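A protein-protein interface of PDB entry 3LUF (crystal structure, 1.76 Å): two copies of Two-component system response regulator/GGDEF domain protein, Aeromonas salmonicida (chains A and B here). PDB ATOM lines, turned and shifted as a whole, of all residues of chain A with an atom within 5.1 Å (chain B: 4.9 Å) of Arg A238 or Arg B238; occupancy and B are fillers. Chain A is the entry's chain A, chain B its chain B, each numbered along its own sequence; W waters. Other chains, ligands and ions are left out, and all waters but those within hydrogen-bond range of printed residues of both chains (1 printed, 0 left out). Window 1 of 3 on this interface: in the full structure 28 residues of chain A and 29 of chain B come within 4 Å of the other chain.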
ATOM      1  N   ILE A 203      18.601 -29.610   1.698  1.00  0.00           N
ATOM      2  CA  ILE A 203      18.424 -28.449   0.818  1.00  0.00           C
ATOM      3  C   ILE A 203      19.823 -28.033   0.390  1.00  0.00           C
ATOM      4  O   ILE A 203      20.698 -27.778   1.248  1.00  0.00           O
ATOM      5  CB  ILE A 203      17.701 -27.255   1.520  1.00  0.00           C
ATOM      6  CG1 ILE A 203      16.280 -27.692   1.951  1.00  0.00           C
ATOM      7  CG2 ILE A 203      17.699 -25.993   0.597  1.00  0.00           C
ATOM      8  CD1 ILE A 203      15.515 -26.675   2.898  1.00  0.00           C
ATOM      9  N   ASP A 224      15.685 -30.229  -2.426  1.00  0.00           N
ATOM     10  CA  ASP A 224      15.369 -28.897  -2.921  1.00  0.00           C
ATOM     11  C   ASP A 224      16.636 -28.058  -2.995  1.00  0.00           C
ATOM     12  O   ASP A 224      17.727 -28.501  -2.581  1.00  0.00           O
ATOM     13  CB  ASP A 224      14.384 -28.235  -1.951  1.00  0.00           C
ATOM     14  CG  ASP A 224      13.418 -27.261  -2.654  1.00  0.00           C
ATOM     15  OD1 ASP A 224      13.713 -26.822  -3.782  1.00  0.00           O
ATOM     16  OD2 ASP A 224      12.348 -26.982  -2.055  1.00  0.00           O
ATOM     17  N   PHE A 225      16.501 -26.866  -3.564  1.00  0.00           N
ATOM     18  CA  PHE A 225      17.619 -25.933  -3.650  1.00  0.00           C
ATOM     19  C   PHE A 225      17.206 -24.588  -3.038  1.00  0.00           C
ATOM     20  O   PHE A 225      16.030 -24.233  -2.999  1.00  0.00           O
ATOM     21  CB  PHE A 225      18.036 -25.726  -5.116  1.00  0.00           C
ATOM     22  CG  PHE A 225      17.023 -24.915  -5.909  1.00  0.00           C
ATOM     23  CD1 PHE A 225      15.909 -25.527  -6.465  1.00  0.00           C
ATOM     24  CD2 PHE A 225      17.176 -23.538  -6.066  1.00  0.00           C
ATOM     25  CE1 PHE A 225      14.944 -24.756  -7.172  1.00  0.00           C
ATOM     26  CE2 PHE A 225      16.230 -22.776  -6.752  1.00  0.00           C
ATOM     27  CZ  PHE A 225      15.112 -23.397  -7.310  1.00  0.00           C
ATOM     28  N   LEU A 226      18.196 -23.795  -2.658  1.00  0.00           N
ATOM     29  CA  LEU A 226      17.960 -22.420  -2.201  1.00  0.00           C
ATOM     30  C   LEU A 226      19.164 -21.621  -2.663  1.00  0.00           C
ATOM     31  O   LEU A 226      20.314 -21.925  -2.285  1.00  0.00           O
ATOM     32  CB  LEU A 226      17.810 -22.366  -0.673  1.00  0.00           C
ATOM     33  CG  LEU A 226      17.639 -20.944  -0.098  1.00  0.00           C
ATOM     34  CD1 LEU A 226      16.330 -20.377  -0.576  1.00  0.00           C
ATOM     35  CD2 LEU A 226      17.659 -20.998   1.448  1.00  0.00           C
ATOM     36  N   GLU A 234      12.564 -16.049   2.350  1.00  0.00           N
ATOM     37  CA  GLU A 234      12.832 -17.057   1.327  1.00  0.00           C
ATOM     38  C   GLU A 234      13.305 -18.337   2.029  1.00  0.00           C
ATOM     39  O   GLU A 234      12.810 -19.438   1.759  1.00  0.00           O
ATOM     40  CB  GLU A 234      13.923 -16.544   0.392  1.00  0.00           C
ATOM     41  CG  GLU A 234      13.486 -15.340  -0.510  1.00  0.00           C
ATOM     42  CD  GLU A 234      14.601 -14.872  -1.436  1.00  0.00           C
ATOM     43  OE1 GLU A 234      15.778 -15.196  -1.192  1.00  0.00           O
ATOM     44  OE2 GLU A 234      14.301 -14.168  -2.423  1.00  0.00           O
ATOM     45  N   LEU A 235      14.253 -18.173   2.943  1.00  0.00           N
ATOM     46  CA  LEU A 235      14.698 -19.301   3.778  1.00  0.00           C
ATOM     47  C   LEU A 235      13.522 -19.974   4.512  1.00  0.00           C
ATOM     48  O   LEU A 235      13.408 -21.190   4.512  1.00  0.00           O
ATOM     49  CB  LEU A 235      15.798 -18.878   4.737  1.00  0.00           C
ATOM     50  CG  LEU A 235      16.343 -19.998   5.670  1.00  0.00           C
ATOM     51  CD1 LEU A 235      17.132 -21.084   4.911  1.00  0.00           C
ATOM     52  CD2 LEU A 235      17.185 -19.404   6.803  1.00  0.00           C
ATOM     53  N   GLN A 236      12.674 -19.179   5.157  1.00  0.00           N
ATOM     54  CA  GLN A 236      11.474 -19.706   5.824  1.00  0.00           C
ATOM     55  C   GLN A 236      10.505 -20.462   4.923  1.00  0.00           C
ATOM     56  O   GLN A 236       9.956 -21.511   5.312  1.00  0.00           O
ATOM     57  CB  GLN A 236      10.756 -18.549   6.518  1.00  0.00           C
ATOM     58  CG  GLN A 236       9.593 -18.967   7.391  1.00  0.00           C
ATOM     59  CD  GLN A 236       9.265 -17.908   8.425  1.00  0.00           C
ATOM     60  OE1 GLN A 236       9.621 -18.042   9.592  1.00  0.00           O
ATOM     61  NE2 GLN A 236       8.609 -16.838   7.998  1.00  0.00           N
ATOM     62  N   CYS A 237      10.273 -19.928   3.732  1.00  0.00           N
ATOM     63  CA  CYS A 237       9.398 -20.583   2.761  1.00  0.00           C
ATOM     64  C   CYS A 237       9.960 -21.963   2.424  1.00  0.00           C
ATOM     65  O   CYS A 237       9.264 -22.992   2.508  1.00  0.00           O
ATOM     66  CB  CYS A 237       9.314 -19.736   1.498  1.00  0.00           C
ATOM     67  SG  CYS A 237       8.390 -20.445   0.208  1.00  0.00           S
ATOM     68  N   ARG A 238      11.244 -21.977   2.087  1.00  0.00           N
ATOM     69  CA  ARG A 238      11.883 -23.185   1.591  1.00  0.00           C
ATOM     70  C   ARG A 238      12.057 -24.229   2.695  1.00  0.00           C
ATOM     71  O   ARG A 238      11.808 -25.423   2.498  1.00  0.00           O
ATOM     72  CB  ARG A 238      13.232 -22.799   0.945  1.00  0.00           C
ATOM     73  CG  ARG A 238      13.795 -23.771  -0.066  1.00  0.00           C
ATOM     74  CD  ARG A 238      12.848 -24.160  -1.201  1.00  0.00           C
ATOM     75  NE  ARG A 238      12.127 -23.083  -1.887  1.00  0.00           N
ATOM     76  CZ  ARG A 238      12.660 -22.224  -2.757  1.00  0.00           C
ATOM     77  NH1 ARG A 238      13.953 -22.275  -3.090  1.00  0.00           N
ATOM     78  NH2 ARG A 238      11.878 -21.312  -3.318  1.00  0.00           N
ATOM     79  N   VAL A 239      12.456 -23.786   3.889  1.00  0.00           N
ATOM     80  CA  VAL A 239      12.597 -24.729   4.996  1.00  0.00           C
ATOM     81  C   VAL A 239      11.245 -25.267   5.414  1.00  0.00           C
ATOM     82  O   VAL A 239      11.087 -26.479   5.597  1.00  0.00           O
ATOM     83  CB  VAL A 239      13.333 -24.079   6.156  1.00  0.00           C
ATOM     84  CG1 VAL A 239      13.210 -24.892   7.449  1.00  0.00           C
ATOM     85  CG2 VAL A 239      14.811 -23.906   5.785  1.00  0.00           C
ATOM     86  N   SER A 240      10.246 -24.375   5.576  1.00  0.00           N
ATOM     87  CA  SER A 240       8.925 -24.843   5.970  1.00  0.00           C
ATOM     88  C   SER A 240       8.361 -25.879   5.012  1.00  0.00           C
ATOM     89  O   SER A 240       7.760 -26.870   5.446  1.00  0.00           O
ATOM     90  CB  SER A 240       7.926 -23.672   6.067  1.00  0.00           C
ATOM     91  OG  SER A 240       8.387 -22.754   7.020  1.00  0.00           O
ATOM     92  N   HIS A 241       8.516 -25.640   3.701  1.00  0.00           N
ATOM     93  CA  HIS A 241       7.915 -26.538   2.745  1.00  0.00           C
ATOM     94  C   HIS A 241       8.548 -27.926   2.875  1.00  0.00           C
ATOM     95  O   HIS A 241       7.860 -28.944   2.835  1.00  0.00           O
ATOM     96  CB  HIS A 241       8.042 -26.040   1.293  1.00  0.00           C
ATOM     97  CG  HIS A 241       7.742 -27.118   0.298  1.00  0.00           C
ATOM     98  ND1 HIS A 241       6.453 -27.459  -0.061  1.00  0.00           N
ATOM     99  CD2 HIS A 241       8.553 -28.000  -0.335  1.00  0.00           C
ATOM    100  CE1 HIS A 241       6.491 -28.459  -0.927  1.00  0.00           C
ATOM    101  NE2 HIS A 241       7.749 -28.828  -1.082  1.00  0.00           N
ATOM    102  N   ASN A 242       9.866 -27.965   3.026  1.00  0.00           N
ATOM    103  CA  ASN A 242      10.565 -29.236   3.171  1.00  0.00           C
ATOM    104  C   ASN A 242      10.296 -29.999   4.459  1.00  0.00           C
ATOM    105  O   ASN A 242      10.153 -31.236   4.441  1.00  0.00           O
ATOM    106  CB  ASN A 242      12.069 -29.041   2.847  1.00  0.00           C
ATOM    107  CG  ASN A 242      12.289 -28.919   1.377  1.00  0.00           C
ATOM    108  OD1 ASN A 242      12.314 -29.939   0.668  1.00  0.00           O
ATOM    109  ND2 ASN A 242      12.373 -27.671   0.864  1.00  0.00           N
ATOM    110  N   ILE B 203       3.242 -19.053  -7.808  1.00  0.00           N
ATOM    111  CA  ILE B 203       4.683 -18.808  -7.654  1.00  0.00           C
ATOM    112  C   ILE B 203       4.981 -17.406  -8.159  1.00  0.00           C
ATOM    113  O   ILE B 203       4.742 -17.083  -9.350  1.00  0.00           O
ATOM    114  CB  ILE B 203       5.553 -19.815  -8.452  1.00  0.00           C
ATOM    115  CG1 ILE B 203       5.172 -21.262  -8.052  1.00  0.00           C
ATOM    116  CG2 ILE B 203       7.039 -19.518  -8.218  1.00  0.00           C
ATOM    117  CD1 ILE B 203       5.784 -22.386  -8.984  1.00  0.00           C
ATOM    118  N   ASP B 224       4.982 -19.649  -3.090  1.00  0.00           N
ATOM    119  CA  ASP B 224       6.409 -19.836  -3.336  1.00  0.00           C
ATOM    120  C   ASP B 224       6.950 -18.679  -4.148  1.00  0.00           C
ATOM    121  O   ASP B 224       6.192 -17.810  -4.637  1.00  0.00           O
ATOM    122  CB  ASP B 224       6.592 -21.152  -4.133  1.00  0.00           C
ATOM    123  CG  ASP B 224       7.926 -21.837  -3.858  1.00  0.00           C
ATOM    124  OD1 ASP B 224       8.860 -21.211  -3.287  1.00  0.00           O
ATOM    125  OD2 ASP B 224       8.047 -23.015  -4.268  1.00  0.00           O
ATOM    126  N   PHE B 225       8.268 -18.668  -4.299  1.00  0.00           N
ATOM    127  CA  PHE B 225       8.951 -17.627  -5.080  1.00  0.00           C
ATOM    128  C   PHE B 225       9.971 -18.265  -5.998  1.00  0.00           C
ATOM    129  O   PHE B 225      10.443 -19.378  -5.734  1.00  0.00           O
ATOM    130  CB  PHE B 225       9.672 -16.649  -4.138  1.00  0.00           C
ATOM    131  CG  PHE B 225      10.875 -17.255  -3.455  1.00  0.00           C
ATOM    132  CD1 PHE B 225      12.146 -17.045  -3.973  1.00  0.00           C
ATOM    133  CD2 PHE B 225      10.726 -18.061  -2.336  1.00  0.00           C
ATOM    134  CE1 PHE B 225      13.260 -17.615  -3.363  1.00  0.00           C
ATOM    135  CE2 PHE B 225      11.848 -18.663  -1.720  1.00  0.00           C
ATOM    136  CZ  PHE B 225      13.117 -18.410  -2.255  1.00  0.00           C
ATOM    137  N   LEU B 226      10.332 -17.547  -7.048  1.00  0.00           N
ATOM    138  CA  LEU B 226      11.376 -18.006  -7.950  1.00  0.00           C
ATOM    139  C   LEU B 226      12.035 -16.755  -8.490  1.00  0.00           C
ATOM    140  O   LEU B 226      11.371 -15.896  -9.087  1.00  0.00           O
ATOM    141  CB  LEU B 226      10.760 -18.867  -9.060  1.00  0.00           C
ATOM    142  CG  LEU B 226      11.674 -19.328 -10.191  1.00  0.00           C
ATOM    143  CD1 LEU B 226      12.767 -20.160  -9.601  1.00  0.00           C
ATOM    144  CD2 LEU B 226      10.818 -20.123 -11.199  1.00  0.00           C
ATOM    145  N   GLU B 234      15.558 -25.551 -12.095  1.00  0.00           N
ATOM    146  CA  GLU B 234      15.059 -24.809 -10.950  1.00  0.00           C
ATOM    147  C   GLU B 234      13.552 -24.582 -11.085  1.00  0.00           C
ATOM    148  O   GLU B 234      12.796 -24.880 -10.156  1.00  0.00           O
ATOM    149  CB  GLU B 234      15.808 -23.503 -10.776  1.00  0.00           C
ATOM    150  CG  GLU B 234      17.228 -23.743 -10.251  1.00  0.00           C
ATOM    151  CD  GLU B 234      18.067 -22.473 -10.220  1.00  0.00           C
ATOM    152  OE1 GLU B 234      19.032 -22.432  -9.424  1.00  0.00           O
ATOM    153  OE2 GLU B 234      17.785 -21.545 -11.013  1.00  0.00           O
ATOM    154  N   LEU B 235      13.127 -24.192 -12.285  1.00  0.00           N
ATOM    155  CA  LEU B 235      11.704 -23.987 -12.564  1.00  0.00           C
ATOM    156  C   LEU B 235      10.955 -25.295 -12.375  1.00  0.00           C
ATOM    157  O   LEU B 235       9.932 -25.323 -11.694  1.00  0.00           O
ATOM    158  CB  LEU B 235      11.463 -23.433 -13.995  1.00  0.00           C
ATOM    159  CG  LEU B 235       9.979 -23.389 -14.404  1.00  0.00           C
ATOM    160  CD1 LEU B 235       9.188 -22.379 -13.589  1.00  0.00           C
ATOM    161  CD2 LEU B 235       9.864 -23.109 -15.883  1.00  0.00           C
ATOM    162  N   GLN B 236      11.452 -26.365 -12.997  1.00  0.00           N
ATOM    163  CA  GLN B 236      10.862 -27.689 -12.827  1.00  0.00           C
ATOM    164  C   GLN B 236      10.726 -28.104 -11.378  1.00  0.00           C
ATOM    165  O   GLN B 236       9.676 -28.576 -10.993  1.00  0.00           O
ATOM    166  CB  GLN B 236      11.641 -28.759 -13.594  1.00  0.00           C
ATOM    167  CG  GLN B 236      11.153 -30.188 -13.319  1.00  0.00           C
ATOM    168  CD  GLN B 236      11.742 -31.203 -14.315  1.00  0.00           C
ATOM    169  OE1 GLN B 236      11.008 -31.883 -15.042  1.00  0.00           O
ATOM    170  NE2 GLN B 236      13.064 -31.253 -14.390  1.00  0.00           N
ATOM    171  N   CYS B 237      11.793 -27.929 -10.581  1.00  0.00           N
ATOM    172  CA  CYS B 237      11.780 -28.306  -9.163  1.00  0.00           C
ATOM    173  C   CYS B 237      10.687 -27.534  -8.421  1.00  0.00           C
ATOM    174  O   CYS B 237       9.921 -28.122  -7.663  1.00  0.00           O
ATOM    175  CB  CYS B 237      13.143 -27.986  -8.534  1.00  0.00           C
ATOM    176  SG  CYS B 237      13.266 -28.276  -6.806  1.00  0.00           S
ATOM    177  N   ARG B 238      10.622 -26.226  -8.646  1.00  0.00           N
ATOM    178  CA  ARG B 238       9.616 -25.421  -7.918  1.00  0.00           C
ATOM    179  C   ARG B 238       8.175 -25.809  -8.287  1.00  0.00           C
ATOM    180  O   ARG B 238       7.279 -25.881  -7.413  1.00  0.00           O
ATOM    181  CB  ARG B 238       9.806 -23.939  -8.242  1.00  0.00           C
ATOM    182  CG  ARG B 238      11.091 -23.375  -7.703  1.00  0.00           C
ATOM    183  CD  ARG B 238      10.916 -22.783  -6.282  1.00  0.00           C
ATOM    184  NE  ARG B 238      10.396 -23.718  -5.289  1.00  0.00           N
ATOM    185  CZ  ARG B 238      11.107 -24.677  -4.691  1.00  0.00           C
ATOM    186  NH1 ARG B 238      12.382 -24.872  -5.027  1.00  0.00           N
ATOM    187  NH2 ARG B 238      10.529 -25.468  -3.789  1.00  0.00           N
ATOM    188  N   VAL B 239       7.970 -25.996  -9.588  1.00  0.00           N
ATOM    189  CA  VAL B 239       6.661 -26.354 -10.092  1.00  0.00           C
ATOM    190  C   VAL B 239       6.280 -27.700  -9.523  1.00  0.00           C
ATOM    191  O   VAL B 239       5.203 -27.832  -8.944  1.00  0.00           O
ATOM    192  CB  VAL B 239       6.582 -26.299 -11.614  1.00  0.00           C
ATOM    193  CG1 VAL B 239       5.300 -27.038 -12.114  1.00  0.00           C
ATOM    194  CG2 VAL B 239       6.591 -24.859 -12.076  1.00  0.00           C
ATOM    195  N   SER B 240       7.190 -28.685  -9.586  1.00  0.00           N
ATOM    196  CA  SER B 240       6.851 -30.003  -9.044  1.00  0.00           C
ATOM    197  C   SER B 240       6.503 -29.943  -7.562  1.00  0.00           C
ATOM    198  O   SER B 240       5.508 -30.533  -7.123  1.00  0.00           O
ATOM    199  CB  SER B 240       7.988 -31.009  -9.276  1.00  0.00           C
ATOM    200  OG  SER B 240       8.136 -31.126 -10.663  1.00  0.00           O
ATOM    201  N   HIS B 241       7.294 -29.192  -6.777  1.00  0.00           N
ATOM    202  CA  HIS B 241       7.030 -29.076  -5.339  1.00  0.00           C
ATOM    203  C   HIS B 241       5.648 -28.475  -5.048  1.00  0.00           C
ATOM    204  O   HIS B 241       4.955 -28.944  -4.130  1.00  0.00           O
ATOM    205  CB  HIS B 241       8.099 -28.246  -4.616  1.00  0.00           C
ATOM    206  CG  HIS B 241       9.338 -29.005  -4.249  1.00  0.00           C
ATOM    207  ND1 HIS B 241       9.351 -29.971  -3.270  1.00  0.00           N
ATOM    208  CD2 HIS B 241      10.617 -28.895  -4.686  1.00  0.00           C
ATOM    209  CE1 HIS B 241      10.585 -30.443  -3.134  1.00  0.00           C
ATOM    210  NE2 HIS B 241      11.365 -29.817  -3.996  1.00  0.00           N
ATOM    211  N   ASN B 242       5.278 -27.455  -5.800  1.00  0.00           N
ATOM    212  CA  ASN B 242       3.970 -26.802  -5.600  1.00  0.00           C
ATOM    213  C   ASN B 242       2.800 -27.689  -6.008  1.00  0.00           C
ATOM    214  O   ASN B 242       1.750 -27.736  -5.315  1.00  0.00           O
ATOM    215  CB  ASN B 242       3.912 -25.437  -6.293  1.00  0.00           C
ATOM    216  CG  ASN B 242       4.665 -24.400  -5.508  1.00  0.00           C
ATOM    217  OD1 ASN B 242       5.869 -24.191  -5.703  1.00  0.00           O
ATOM    218  ND2 ASN B 242       4.005 -23.854  -4.503  1.00  0.00           N
HETATM  219  O   HOH W   1      13.126 -20.334  -5.685  1.00  0.00           O
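Of the printed residues of chain B, Asp A224 touches Cys B237 (3.4 Å), Arg B238 (2.7 Å) and His B241 (3.5 Å). Of the printed residues of chain B, Glu A234 touches Phe B225. Arg A238 touches just these residues of chain B: Asp B224, Phe B225 and Arg B238. Val A239 touches none of the printed residues of chain B. Of the printed residues of chain A, Glu B234 touches Phe A225. Arg B238 touches three residues of chain A. Of the printed residues of chain A, His B241 touches Asp A224 and His A241. The nearest printed residue of chain B that does not touch Arg A238 is Leu B226 (5.5 Å).
CG of Asp A224 touches NE2 of His B241 (3.5 Å). Glu B234 touches Phe A225. CD1 of Phe A225 touches SG of Cys B237 (3.8 Å). Arg B238 touches Phe A225 (NH1 to CE1, 3.3 Å). CB of Glu A234 touches CZ of Phe B225, at 3.3 Å.
Water W1 bridges O of Phe B225 (2.8 Å) and NH2 of Arg A238 (2.8 Å).
The guanidinium group (NH2) of Arg B238 sits close to the guanidinium group (NE) of Arg A238, at 3.4 Å. SG of Cys A237 lies within hydrogen-bond range of OD1 of Asp B224 (3.6 Å). NH2 of Arg A238 lies within salt-bridge range of OD1 of Asp B224, at 3.0 Å. NE2 of His A241 sits at hydrogen-bond distance from ND1 of His B241. The backbone carbonyl oxygen of Phe B225 sits close to the guanidinium group of Arg A238 (3.4 Å). The guanidinium group (NH1) of Arg B238 is in salt-bridge range of the side-chain carboxylate (OD1) of Asp A224 (2.7 Å). The side-chain carboxylate (OD1) of Asp A224 is in hydrogen-bond range of the side-chain sulfur (SG) of Cys B237 (3.4 Å).
Asp A224 touches His B241, but with the chains exchanged His A241 does not touch Asp B224 (6.1 Å). Phe A225 touches Cys B237, but with the chains exchanged Cys A237 does not touch Phe B225 (4.2 Å). Arg A238 touches its own counterpart, Arg B238. His B241 touches its own counterpart, His A241. Positions printed for both chains: 203, 224, 225, 226, 234, 235, 236, 237, 238, 239, 240, 241 and 242. Of the 12 pairs that touch across the chains among the printed residues, 10 have their exchanged pair printed and touching as well.
Of the 13 printed residues of chain A, 6 touch a printed residue of chain B. Hydrophobic or aromatic side chains of chain B that line the printed part of chain A: Phe B225 and His B241. Among the printed residues, Asp or Glu carboxylates within 4 Å of a Lys or Arg side-chain nitrogen of the other chain: Asp A224 with Arg B238 and Arg A238 with Asp B224.
OD2 of Asp A224 is in salt-bridge range of NE of Arg A238 (3.9 Å). NE2 of His B241 lies close to SG of Cys B237 (3.7 Å). OD1 of Asn B242 lies close to O of Arg B238, 2.8 Å away. The side-chain amide oxygen (OD1) of Asn B242 sits close to the side-chain carboxylate (OD2) of Asp B224 (2.9 Å). O of Arg A238 is in hydrogen-bond range of ND2 of Asn A242 (2.8 Å). The side-chain carboxylate (OD2) of Asp A224 sits at hydrogen-bond distance from the side-chain amide nitrogen (ND2) of Asn A242 (3.0 Å).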
